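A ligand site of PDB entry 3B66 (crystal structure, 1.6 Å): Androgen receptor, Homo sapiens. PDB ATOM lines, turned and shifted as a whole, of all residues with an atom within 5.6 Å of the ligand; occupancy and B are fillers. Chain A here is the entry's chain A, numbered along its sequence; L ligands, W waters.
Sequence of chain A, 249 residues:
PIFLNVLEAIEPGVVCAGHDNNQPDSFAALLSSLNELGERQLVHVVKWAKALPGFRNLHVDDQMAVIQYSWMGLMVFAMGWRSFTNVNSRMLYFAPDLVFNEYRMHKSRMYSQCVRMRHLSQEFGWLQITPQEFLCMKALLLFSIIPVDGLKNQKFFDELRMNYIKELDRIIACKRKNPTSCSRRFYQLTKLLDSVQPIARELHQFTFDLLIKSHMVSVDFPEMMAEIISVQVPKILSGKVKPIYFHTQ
Water W1 lies within hydrogen-bond range of O of Met 75 (2.8 Å), NE2 of Gln 41 (2.8 Å), NH2 of Arg 82 (2.9 Å) and N3 of the ligand (3.1 Å).
The backbone NH (N) of Val 76 lies close to a fluorine (F1) of the ligand, 3.2 Å away. A fluorine (F3) of the ligand sits close to the side-chain sulfur (SD) of Met 117, 3.7 Å away. The side-chain sulfur of Met 225 lies close to an oxygen (O3) of the ligand, at 3.6 Å. Residues that only touch the ligand: Val 233 (3.0 Å), Trp 71 (3.2 Å), Met 79 (3.3 Å), Met 75 (3.3 Å), Ile 228 (3.4 Å), Thr 207 (3.4 Å), Leu 203 (3.4 Å), Phe 94 (3.4 Å), Gln 68 (3.5 Å), Ile 229 (3.7 Å), Gly 38 (3.7 Å), Leu 37 (3.8 Å), His 204 (3.8 Å) and Leu 31 (3.8 Å). Of the 30 residues printed, 22 come within 4 Å of the ligand.
The side-chain sulfur (SD) of Met 75 sits close to the side-chain amide nitrogen (NE2) of Gln 41 (3.2 Å). The backbone carbonyl oxygen (O) of Ile 228 lies within hydrogen-bond range of the backbone NH (N) of Val 233 (3.1 Å). The backbone carbonyl oxygen (O) of Phe 94 sits at hydrogen-bond distance from the guanidinium group (NH2) of Arg 82, 3.0 Å away. The side-chain hydroxyl of Thr 207 is in hydrogen-bond range of the backbone carbonyl oxygen of Leu 203, at 2.6 Å. O of Leu 31 sits close to ND2 of Asn 35 (3.5 Å). SD of Met 75 lies close to NE1 of Trp 71, 3.3 Å away. The indole nitrogen (NE1) of Trp 71 sits close to the backbone carbonyl oxygen (O) of Gly 38 (3.4 Å). OD1 of Asn 35 sits close to SD of Met 225, 3.6 Å away.
A nitrogen (N3) of the ligand sits close to the side-chain amide oxygen of Gln 41 (3.5 Å). OD1 of Asn 35 sits at hydrogen-bond distance from O4 of the ligand (2.6 Å). NH2 of Arg 82 lies within hydrogen-bond range of N3 of the ligand. The backbone NH of Asn 35 is in hydrogen-bond range of an oxygen (O4) of the ligand, 3.1 Å away. The backbone carbonyl oxygen (O) of Leu 34 lies close to an oxygen (O4) of the ligand. The backbone NH (N) of Met 72 sits at hydrogen-bond distance from an oxygen (O2) of the ligand (3.3 Å).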
ATOM      1  N   LEU A  31       6.779  16.757 -19.439  1.00  0.00           N
ATOM      2  CA  LEU A  31       6.631  17.475 -20.705  1.00  0.00           C
ATOM      3  C   LEU A  31       5.952  18.831 -20.543  1.00  0.00           C
ATOM      4  O   LEU A  31       6.303  19.792 -21.230  1.00  0.00           O
ATOM      5  CB  LEU A  31       5.877  16.597 -21.724  1.00  0.00           C
ATOM      6  CG  LEU A  31       6.770  15.776 -22.661  1.00  0.00           C
ATOM      7  CD1 LEU A  31       7.559  16.703 -23.566  1.00  0.00           C
ATOM      8  CD2 LEU A  31       7.714  14.881 -21.857  1.00  0.00           C
ATOM      9  N   LEU A  34       8.632  20.991 -19.456  1.00  0.00           N
ATOM     10  CA  LEU A  34       9.572  21.296 -20.523  1.00  0.00           C
ATOM     11  C   LEU A  34       8.944  22.348 -21.427  1.00  0.00           C
ATOM     12  O   LEU A  34       9.611  23.285 -21.858  1.00  0.00           O
ATOM     13  CB  LEU A  34       9.894  20.031 -21.335  1.00  0.00           C
ATOM     14  CG  LEU A  34      10.962  19.103 -20.729  1.00  0.00           C
ATOM     15  CD1 LEU A  34      11.043  17.810 -21.539  1.00  0.00           C
ATOM     16  CD2 LEU A  34      12.322  19.806 -20.691  1.00  0.00           C
ATOM     17  N   ASN A  35       7.644  22.218 -21.697  1.00  0.00           N
ATOM     18  CA  ASN A  35       6.939  23.189 -22.542  1.00  0.00           C
ATOM     19  C   ASN A  35       6.949  24.571 -21.910  1.00  0.00           C
ATOM     20  O   ASN A  35       7.260  25.562 -22.576  1.00  0.00           O
ATOM     21  CB  ASN A  35       5.482  22.767 -22.771  1.00  0.00           C
ATOM     22  CG  ASN A  35       5.362  21.582 -23.700  1.00  0.00           C
ATOM     23  OD1 ASN A  35       6.302  21.231 -24.418  1.00  0.00           O
ATOM     24  ND2 ASN A  35       4.191  20.956 -23.704  1.00  0.00           N
ATOM     25  N   GLU A  36       6.605  24.625 -20.626  1.00  0.00           N
ATOM     26  CA  GLU A  36       6.579  25.893 -19.882  1.00  0.00           C
ATOM     27  C   GLU A  36       7.976  26.505 -19.838  1.00  0.00           C
ATOM     28  O   GLU A  36       8.126  27.701 -20.046  1.00  0.00           O
ATOM     29  CB  GLU A  36       6.067  25.658 -18.453  1.00  0.00           C
ATOM     30  CG  GLU A  36       6.186  26.880 -17.534  1.00  0.00           C
ATOM     31  CD  GLU A  36       5.259  28.029 -17.919  1.00  0.00           C
ATOM     32  OE1 GLU A  36       5.520  29.172 -17.486  1.00  0.00           O
ATOM     33  OE2 GLU A  36       4.251  27.799 -18.633  1.00  0.00           O
ATOM     34  N   LEU A  37       8.978  25.672 -19.580  1.00  0.00           N
ATOM     35  CA  LEU A  37      10.360  26.170 -19.538  1.00  0.00           C
ATOM     36  C   LEU A  37      10.759  26.665 -20.921  1.00  0.00           C
ATOM     37  O   LEU A  37      11.472  27.677 -21.049  1.00  0.00           O
ATOM     38  CB  LEU A  37      11.316  25.049 -19.102  1.00  0.00           C
ATOM     39  CG  LEU A  37      12.791  25.462 -19.109  1.00  0.00           C
ATOM     40  CD1 LEU A  37      13.027  26.584 -18.082  1.00  0.00           C
ATOM     41  CD2 LEU A  37      13.664  24.250 -18.801  1.00  0.00           C
ATOM     42  N   GLY A  38      10.311  25.959 -21.952  1.00  0.00           N
ATOM     43  CA  GLY A  38      10.639  26.381 -23.307  1.00  0.00           C
ATOM     44  C   GLY A  38      10.122  27.782 -23.560  1.00  0.00           C
ATOM     45  O   GLY A  38      10.847  28.635 -24.054  1.00  0.00           O
ATOM     46  N   GLN A  41      12.037  30.482 -21.582  1.00  0.00           N
ATOM     47  CA  GLN A  41      13.323  30.782 -22.199  1.00  0.00           C
ATOM     48  C   GLN A  41      13.148  31.619 -23.462  1.00  0.00           C
ATOM     49  O   GLN A  41      13.926  32.536 -23.712  1.00  0.00           O
ATOM     50  CB  GLN A  41      14.103  29.496 -22.503  1.00  0.00           C
ATOM     51  CG  GLN A  41      14.509  28.720 -21.243  1.00  0.00           C
ATOM     52  CD  GLN A  41      15.603  27.688 -21.480  1.00  0.00           C
ATOM     53  OE1 GLN A  41      15.903  26.890 -20.587  1.00  0.00           O
ATOM     54  NE2 GLN A  41      16.213  27.714 -22.660  1.00  0.00           N
ATOM     55  N   GLN A  68      12.552  32.353 -34.127  1.00  0.00           N
ATOM     56  CA  GLN A  68      11.697  31.177 -34.035  1.00  0.00           C
ATOM     57  C   GLN A  68      12.353  29.931 -34.621  1.00  0.00           C
ATOM     58  O   GLN A  68      12.268  28.852 -34.024  1.00  0.00           O
ATOM     59  CB  GLN A  68      10.350  31.478 -34.707  1.00  0.00           C
ATOM     60  CG  GLN A  68       9.612  32.661 -34.048  1.00  0.00           C
ATOM     61  CD  GLN A  68       8.190  32.859 -34.552  1.00  0.00           C
ATOM     62  OE1 GLN A  68       7.877  32.557 -35.701  1.00  0.00           O
ATOM     63  NE2 GLN A  68       7.342  33.425 -33.697  1.00  0.00           N
ATOM     64  N   TYR A  69      13.033  30.055 -35.758  1.00  0.00           N
ATOM     65  CA  TYR A  69      13.690  28.883 -36.350  1.00  0.00           C
ATOM     66  C   TYR A  69      14.849  28.397 -35.464  1.00  0.00           C
ATOM     67  O   TYR A  69      15.049  27.197 -35.315  1.00  0.00           O
ATOM     68  CB  TYR A  69      14.265  29.194 -37.740  1.00  0.00           C
ATOM     69  CG  TYR A  69      13.266  29.641 -38.786  1.00  0.00           C
ATOM     70  CD1 TYR A  69      11.998  29.060 -38.874  1.00  0.00           C
ATOM     71  CD2 TYR A  69      13.596  30.636 -39.703  1.00  0.00           C
ATOM     72  CE1 TYR A  69      11.091  29.460 -39.863  1.00  0.00           C
ATOM     73  CE2 TYR A  69      12.702  31.040 -40.687  1.00  0.00           C
ATOM     74  CZ  TYR A  69      11.455  30.448 -40.757  1.00  0.00           C
ATOM     75  OH  TYR A  69      10.573  30.851 -41.730  1.00  0.00           O
ATOM     76  N   SER A  70      15.585  29.338 -34.882  1.00  0.00           N
ATOM     77  CA  SER A  70      16.736  28.989 -34.042  1.00  0.00           C
ATOM     78  C   SER A  70      16.447  28.667 -32.580  1.00  0.00           C
ATOM     79  O   SER A  70      17.316  28.165 -31.864  1.00  0.00           O
ATOM     80  CB  SER A  70      17.762  30.115 -34.100  1.00  0.00           C
ATOM     81  OG  SER A  70      18.402  30.114 -35.363  1.00  0.00           O
ATOM     82  N   TRP A  71      15.229  28.938 -32.146  1.00  0.00           N
ATOM     83  CA  TRP A  71      14.820  28.720 -30.761  1.00  0.00           C
ATOM     84  C   TRP A  71      15.287  27.391 -30.149  1.00  0.00           C
ATOM     85  O   TRP A  71      15.974  27.392 -29.126  1.00  0.00           O
ATOM     86  CB  TRP A  71      13.292  28.851 -30.686  1.00  0.00           C
ATOM     87  CG  TRP A  71      12.664  28.674 -29.346  1.00  0.00           C
ATOM     88  CD1 TRP A  71      13.269  28.740 -28.123  1.00  0.00           C
ATOM     89  CD2 TRP A  71      11.270  28.444 -29.089  1.00  0.00           C
ATOM     90  NE1 TRP A  71      12.340  28.573 -27.112  1.00  0.00           N
ATOM     91  CE2 TRP A  71      11.105  28.389 -27.689  1.00  0.00           C
ATOM     92  CE3 TRP A  71      10.147  28.283 -29.908  1.00  0.00           C
ATOM     93  CZ2 TRP A  71       9.855  28.175 -27.078  1.00  0.00           C
ATOM     94  CZ3 TRP A  71       8.906  28.072 -29.307  1.00  0.00           C
ATOM     95  CH2 TRP A  71       8.774  28.022 -27.914  1.00  0.00           C
ATOM     96  N   MET A  72      14.927  26.273 -30.759  1.00  0.00           N
ATOM     97  CA  MET A  72      15.303  24.967 -30.225  1.00  0.00           C
ATOM     98  C   MET A  72      16.825  24.793 -30.143  1.00  0.00           C
ATOM     99  O   MET A  72      17.356  24.417 -29.107  1.00  0.00           O
ATOM    100  CB  MET A  72      14.706  23.857 -31.098  1.00  0.00           C
ATOM    101  CG  MET A  72      14.940  22.435 -30.560  1.00  0.00           C
ATOM    102  SD  MET A  72      14.039  22.123 -29.037  1.00  0.00           S
ATOM    103  CE  MET A  72      12.425  21.559 -29.707  1.00  0.00           C
ATOM    104  N   MET A  75      18.521  26.834 -27.385  1.00  0.00           N
ATOM    105  CA  MET A  75      18.304  26.278 -26.064  1.00  0.00           C
ATOM    106  C   MET A  75      19.149  25.026 -25.841  1.00  0.00           C
ATOM    107  O   MET A  75      19.689  24.824 -24.756  1.00  0.00           O
ATOM    108  CB  MET A  75      16.830  25.947 -25.840  1.00  0.00           C
ATOM    109  CG  MET A  75      15.929  27.165 -25.736  1.00  0.00           C
ATOM    110  SD  MET A  75      14.276  26.753 -25.077  1.00  0.00           S
ATOM    111  CE  MET A  75      13.626  25.719 -26.366  1.00  0.00           C
ATOM    112  N   VAL A  76      19.269  24.202 -26.878  1.00  0.00           N
ATOM    113  CA  VAL A  76      20.061  22.973 -26.806  1.00  0.00           C
ATOM    114  C   VAL A  76      21.517  23.297 -26.475  1.00  0.00           C
ATOM    115  O   VAL A  76      22.117  22.687 -25.594  1.00  0.00           O
ATOM    116  CB  VAL A  76      20.023  22.202 -28.156  1.00  0.00           C
ATOM    117  CG1 VAL A  76      21.101  21.130 -28.184  1.00  0.00           C
ATOM    118  CG2 VAL A  76      18.642  21.569 -28.368  1.00  0.00           C
ATOM    119  N   MET A  79      21.876  24.712 -22.940  1.00  0.00           N
ATOM    120  CA  MET A  79      21.587  23.677 -21.964  1.00  0.00           C
ATOM    121  C   MET A  79      22.816  22.756 -21.825  1.00  0.00           C
ATOM    122  O   MET A  79      23.185  22.368 -20.719  1.00  0.00           O
ATOM    123  CB  MET A  79      20.340  22.874 -22.379  1.00  0.00           C
ATOM    124  CG  MET A  79      19.781  21.955 -21.276  1.00  0.00           C
ATOM    125  SD  MET A  79      20.630  20.379 -21.180  1.00  0.00           S
ATOM    126  CE  MET A  79      19.780  19.459 -22.479  1.00  0.00           C
ATOM    127  N   ARG A  82      25.375  24.494 -19.701  1.00  0.00           N
ATOM    128  CA  ARG A  82      24.981  24.483 -18.292  1.00  0.00           C
ATOM    129  C   ARG A  82      25.221  23.125 -17.653  1.00  0.00           C
ATOM    130  O   ARG A  82      25.612  23.045 -16.482  1.00  0.00           O
ATOM    131  CB  ARG A  82      23.504  24.834 -18.130  1.00  0.00           C
ATOM    132  CG  ARG A  82      23.154  26.292 -18.378  1.00  0.00           C
ATOM    133  CD  ARG A  82      21.766  26.598 -17.825  1.00  0.00           C
ATOM    134  NE  ARG A  82      20.707  25.826 -18.485  1.00  0.00           N
ATOM    135  CZ  ARG A  82      20.159  26.158 -19.658  1.00  0.00           C
ATOM    136  NH1 ARG A  82      20.562  27.229 -20.307  1.00  0.00           N
ATOM    137  NH2 ARG A  82      19.196  25.403 -20.172  1.00  0.00           N
ATOM    138  N   TYR A  93      21.123  19.695 -17.329  1.00  0.00           N
ATOM    139  CA  TYR A  93      20.649  20.828 -16.540  1.00  0.00           C
ATOM    140  C   TYR A  93      19.719  21.734 -17.347  1.00  0.00           C
ATOM    141  O   TYR A  93      20.129  22.829 -17.760  1.00  0.00           O
ATOM    142  CB  TYR A  93      21.853  21.623 -16.057  1.00  0.00           C
ATOM    143  CG  TYR A  93      21.637  22.464 -14.820  1.00  0.00           C
ATOM    144  CD1 TYR A  93      21.925  21.959 -13.556  1.00  0.00           C
ATOM    145  CD2 TYR A  93      21.217  23.790 -14.934  1.00  0.00           C
ATOM    146  CE1 TYR A  93      21.795  22.762 -12.421  1.00  0.00           C
ATOM    147  CE2 TYR A  93      21.097  24.590 -13.800  1.00  0.00           C
ATOM    148  CZ  TYR A  93      21.391  24.081 -12.552  1.00  0.00           C
ATOM    149  OH  TYR A  93      21.324  24.898 -11.453  1.00  0.00           O
ATOM    150  N   PHE A  94      18.484  21.310 -17.578  1.00  0.00           N
ATOM    151  CA  PHE A  94      17.529  22.141 -18.331  1.00  0.00           C
ATOM    152  C   PHE A  94      17.285  23.432 -17.544  1.00  0.00           C
ATOM    153  O   PHE A  94      17.167  24.528 -18.116  1.00  0.00           O
ATOM    154  CB  PHE A  94      16.199  21.428 -18.541  1.00  0.00           C
ATOM    155  CG  PHE A  94      16.260  20.262 -19.495  1.00  0.00           C
ATOM    156  CD1 PHE A  94      16.569  18.987 -19.029  1.00  0.00           C
ATOM    157  CD2 PHE A  94      16.005  20.442 -20.848  1.00  0.00           C
ATOM    158  CE1 PHE A  94      16.613  17.895 -19.913  1.00  0.00           C
ATOM    159  CE2 PHE A  94      16.040  19.365 -21.746  1.00  0.00           C
ATOM    160  CZ  PHE A  94      16.352  18.097 -21.273  1.00  0.00           C
ATOM    161  N   MET A 110      12.173  11.046 -24.588  1.00  0.00           N
ATOM    162  CA  MET A 110      13.086  11.814 -25.419  1.00  0.00           C
ATOM    163  C   MET A 110      14.495  11.316 -25.128  1.00  0.00           C
ATOM    164  O   MET A 110      15.458  12.084 -25.216  1.00  0.00           O
ATOM    165  CB  MET A 110      13.016  13.300 -25.054  1.00  0.00           C
ATOM    166  CG  MET A 110      11.640  13.904 -25.056  1.00  0.00           C
ATOM    167  SD  MET A 110      11.672  15.545 -24.334  1.00  0.00           S
ATOM    168  CE  MET A 110      12.307  16.469 -25.670  1.00  0.00           C
ATOM    169  N   MET A 117      22.446  15.159 -26.336  1.00  0.00           N
ATOM    170  CA  MET A 117      22.742  16.426 -25.688  1.00  0.00           C
ATOM    171  C   MET A 117      23.765  16.219 -24.566  1.00  0.00           C
ATOM    172  O   MET A 117      24.550  17.107 -24.264  1.00  0.00           O
ATOM    173  CB  MET A 117      21.460  17.084 -25.157  1.00  0.00           C
ATOM    174  CG  MET A 117      20.510  17.524 -26.270  1.00  0.00           C
ATOM    175  SD  MET A 117      19.064  18.486 -25.751  1.00  0.00           S
ATOM    176  CE  MET A 117      18.080  17.224 -24.995  1.00  0.00           C
ATOM    177  N   LEU A 203      14.448  16.914 -31.910  1.00  0.00           N
ATOM    178  CA  LEU A 203      13.538  17.510 -30.922  1.00  0.00           C
ATOM    179  C   LEU A 203      12.339  18.142 -31.629  1.00  0.00           C
ATOM    180  O   LEU A 203      11.212  18.079 -31.122  1.00  0.00           O
ATOM    181  CB  LEU A 203      14.284  18.536 -30.080  1.00  0.00           C
ATOM    182  CG  LEU A 203      15.326  17.962 -29.105  1.00  0.00           C
ATOM    183  CD1 LEU A 203      16.165  19.078 -28.544  1.00  0.00           C
ATOM    184  CD2 LEU A 203      14.637  17.194 -27.980  1.00  0.00           C
ATOM    185  N   HIS A 204      12.573  18.754 -32.778  1.00  0.00           N
ATOM    186  CA  HIS A 204      11.479  19.348 -33.548  1.00  0.00           C
ATOM    187  C   HIS A 204      10.479  18.270 -33.949  1.00  0.00           C
ATOM    188  O   HIS A 204       9.271  18.456 -33.836  1.00  0.00           O
ATOM    189  CB  HIS A 204      12.006  20.023 -34.820  1.00  0.00           C
ATOM    190  CG  HIS A 204      12.527  21.411 -34.599  1.00  0.00           C
ATOM    191  ND1 HIS A 204      13.630  21.904 -35.266  1.00  0.00           N
ATOM    192  CD2 HIS A 204      12.093  22.424 -33.801  1.00  0.00           C
ATOM    193  CE1 HIS A 204      13.850  23.154 -34.891  1.00  0.00           C
ATOM    194  NE2 HIS A 204      12.924  23.487 -34.009  1.00  0.00           N
ATOM    195  N   PHE A 206      10.019  15.326 -32.550  1.00  0.00           N
ATOM    196  CA  PHE A 206       9.365  14.833 -31.346  1.00  0.00           C
ATOM    197  C   PHE A 206       8.291  15.807 -30.898  1.00  0.00           C
ATOM    198  O   PHE A 206       7.165  15.406 -30.631  1.00  0.00           O
ATOM    199  CB  PHE A 206      10.402  14.643 -30.234  1.00  0.00           C
ATOM    200  CG  PHE A 206       9.803  14.409 -28.874  1.00  0.00           C
ATOM    201  CD1 PHE A 206       9.534  15.479 -28.021  1.00  0.00           C
ATOM    202  CD2 PHE A 206       9.494  13.124 -28.453  1.00  0.00           C
ATOM    203  CE1 PHE A 206       8.964  15.272 -26.778  1.00  0.00           C
ATOM    204  CE2 PHE A 206       8.921  12.898 -27.200  1.00  0.00           C
ATOM    205  CZ  PHE A 206       8.653  13.980 -26.362  1.00  0.00           C
ATOM    206  N   THR A 207       8.647  17.089 -30.821  1.00  0.00           N
ATOM    207  CA  THR A 207       7.712  18.109 -30.391  1.00  0.00           C
ATOM    208  C   THR A 207       6.500  18.174 -31.318  1.00  0.00           C
ATOM    209  O   THR A 207       5.374  18.312 -30.857  1.00  0.00           O
ATOM    210  CB  THR A 207       8.374  19.502 -30.337  1.00  0.00           C
ATOM    211  OG1 THR A 207       9.583  19.429 -29.582  1.00  0.00           O
ATOM    212  CG2 THR A 207       7.441  20.495 -29.673  1.00  0.00           C
ATOM    213  N   LEU A 210       4.273  15.166 -30.765  1.00  0.00           N
ATOM    214  CA  LEU A 210       3.607  15.311 -29.480  1.00  0.00           C
ATOM    215  C   LEU A 210       2.426  16.273 -29.544  1.00  0.00           C
ATOM    216  O   LEU A 210       1.349  15.983 -29.022  1.00  0.00           O
ATOM    217  CB  LEU A 210       4.617  15.783 -28.409  1.00  0.00           C
ATOM    218  CG  LEU A 210       4.099  15.833 -26.972  1.00  0.00           C
ATOM    219  CD1 LEU A 210       3.466  14.492 -26.602  1.00  0.00           C
ATOM    220  CD2 LEU A 210       5.245  16.168 -26.027  1.00  0.00           C
ATOM    221  N   PHE A 221       0.355  22.418 -23.967  1.00  0.00           N
ATOM    222  CA  PHE A 221       1.205  23.274 -24.771  1.00  0.00           C
ATOM    223  C   PHE A 221       0.768  24.712 -24.644  1.00  0.00           C
ATOM    224  O   PHE A 221      -0.400  25.037 -24.841  1.00  0.00           O
ATOM    225  CB  PHE A 221       1.165  22.886 -26.253  1.00  0.00           C
ATOM    226  CG  PHE A 221       2.051  21.727 -26.604  1.00  0.00           C
ATOM    227  CD1 PHE A 221       1.557  20.435 -26.607  1.00  0.00           C
ATOM    228  CD2 PHE A 221       3.386  21.942 -26.927  1.00  0.00           C
ATOM    229  CE1 PHE A 221       2.376  19.357 -26.936  1.00  0.00           C
ATOM    230  CE2 PHE A 221       4.218  20.875 -27.260  1.00  0.00           C
ATOM    231  CZ  PHE A 221       3.714  19.586 -27.261  1.00  0.00           C
ATOM    232  N   MET A 225       3.826  28.563 -28.003  1.00  0.00           N
ATOM    233  CA  MET A 225       4.594  27.411 -28.482  1.00  0.00           C
ATOM    234  C   MET A 225       3.819  26.617 -29.525  1.00  0.00           C
ATOM    235  O   MET A 225       4.382  26.226 -30.552  1.00  0.00           O
ATOM    236  CB  MET A 225       4.978  26.516 -27.316  1.00  0.00           C
ATOM    237  CG  MET A 225       5.818  25.311 -27.719  1.00  0.00           C
ATOM    238  SD  MET A 225       6.286  24.326 -26.287  1.00  0.00           S
ATOM    239  CE  MET A 225       7.651  25.336 -25.638  1.00  0.00           C
ATOM    240  N   ILE A 228       3.886  28.321 -32.907  1.00  0.00           N
ATOM    241  CA  ILE A 228       5.191  28.182 -33.551  1.00  0.00           C
ATOM    242  C   ILE A 228       5.423  26.755 -34.063  1.00  0.00           C
ATOM    243  O   ILE A 228       6.008  26.566 -35.133  1.00  0.00           O
ATOM    244  CB  ILE A 228       6.317  28.570 -32.577  1.00  0.00           C
ATOM    245  CG1 ILE A 228       6.247  30.087 -32.316  1.00  0.00           C
ATOM    246  CG2 ILE A 228       7.662  28.171 -33.143  1.00  0.00           C
ATOM    247  CD1 ILE A 228       7.201  30.582 -31.243  1.00  0.00           C
ATOM    248  N   ILE A 229       4.992  25.767 -33.300  1.00  0.00           N
ATOM    249  CA  ILE A 229       5.169  24.371 -33.702  1.00  0.00           C
ATOM    250  C   ILE A 229       4.316  24.061 -34.941  1.00  0.00           C
ATOM    251  O   ILE A 229       4.742  23.307 -35.816  1.00  0.00           O
ATOM    252  CB  ILE A 229       4.756  23.398 -32.581  1.00  0.00           C
ATOM    253  CG1 ILE A 229       5.675  23.560 -31.365  1.00  0.00           C
ATOM    254  CG2 ILE A 229       4.835  21.956 -33.090  1.00  0.00           C
ATOM    255  CD1 ILE A 229       5.223  22.777 -30.136  1.00  0.00           C
ATOM    256  N   VAL A 233       7.803  25.157 -37.297  1.00  0.00           N
ATOM    257  CA  VAL A 233       8.441  23.838 -37.279  1.00  0.00           C
ATOM    258  C   VAL A 233       8.185  22.987 -38.526  1.00  0.00           C
ATOM    259  O   VAL A 233       9.098  22.312 -39.016  1.00  0.00           O
ATOM    260  CB  VAL A 233       8.029  23.063 -36.015  1.00  0.00           C
ATOM    261  CG1 VAL A 233       8.607  21.649 -36.050  1.00  0.00           C
ATOM    262  CG2 VAL A 233       8.524  23.799 -34.780  1.00  0.00           C
HETATM  263  C1  LIG L   1      10.980  24.308 -28.122  1.00  0.00           C
HETATM  264  C2  LIG L   1      11.211  24.974 -29.318  1.00  0.00           C
HETATM  265  C3  LIG L   1      10.293  24.887 -30.359  1.00  0.00           C
HETATM  266  N1  LIG L   1      10.524  25.492 -31.514  1.00  0.00           N
HETATM  267  O1  LIG L   1       9.557  25.456 -32.556  1.00  0.00           O
HETATM  268  O2  LIG L   1      11.727  26.237 -31.708  1.00  0.00           O
HETATM  269  C4  LIG L   1       9.144  24.124 -30.189  1.00  0.00           C
HETATM  270  C5  LIG L   1       8.913  23.452 -28.986  1.00  0.00           C
HETATM  271  C6  LIG L   1       9.831  23.545 -27.952  1.00  0.00           C
HETATM  272  O3  LIG L   1       9.612  22.945 -26.743  1.00  0.00           O
HETATM  273  C7  LIG L   1       9.166  21.589 -26.845  1.00  0.00           C
HETATM  274  C8  LIG L   1       9.583  20.872 -25.562  1.00  0.00           C
HETATM  275  O4  LIG L   1       8.877  21.440 -24.455  1.00  0.00           O
HETATM  276  C9  LIG L   1       9.270  19.378 -25.688  1.00  0.00           C
HETATM  277  C10 LIG L   1      11.084  21.076 -25.362  1.00  0.00           C
HETATM  278  O5  LIG L   1      11.908  20.521 -26.082  1.00  0.00           O
HETATM  279  N2  LIG L   1      11.370  21.946 -24.390  1.00  0.00           N
HETATM  280  C11 LIG L   1      12.586  22.317 -23.999  1.00  0.00           C
HETATM  281  C12 LIG L   1      13.762  21.853 -24.575  1.00  0.00           C
HETATM  282  C13 LIG L   1      12.667  23.240 -22.960  1.00  0.00           C
HETATM  283  C14 LIG L   1      13.913  23.676 -22.515  1.00  0.00           C
HETATM  284  C15 LIG L   1      15.078  23.190 -23.109  1.00  0.00           C
HETATM  285  C16 LIG L   1      16.310  23.708 -22.588  1.00  0.00           C
HETATM  286  N3  LIG L   1      17.280  24.124 -22.163  1.00  0.00           N
HETATM  287  C17 LIG L   1      15.020  22.275 -24.153  1.00  0.00           C
HETATM  288  C18 LIG L   1      16.275  21.746 -24.878  1.00  0.00           C
HETATM  289  F1  LIG L   1      16.660  22.613 -25.803  1.00  0.00           F
HETATM  290  F2  LIG L   1      17.306  21.533 -24.053  1.00  0.00           F
HETATM  291  F3  LIG L   1      16.059  20.573 -25.484  1.00  0.00           F
HETATM  292  O   HOH W   1      18.873  26.707 -22.797  1.00  0.00           O
HETATM  293  O   HOH W   2      13.475  26.239 -33.360  1.00  0.00           O
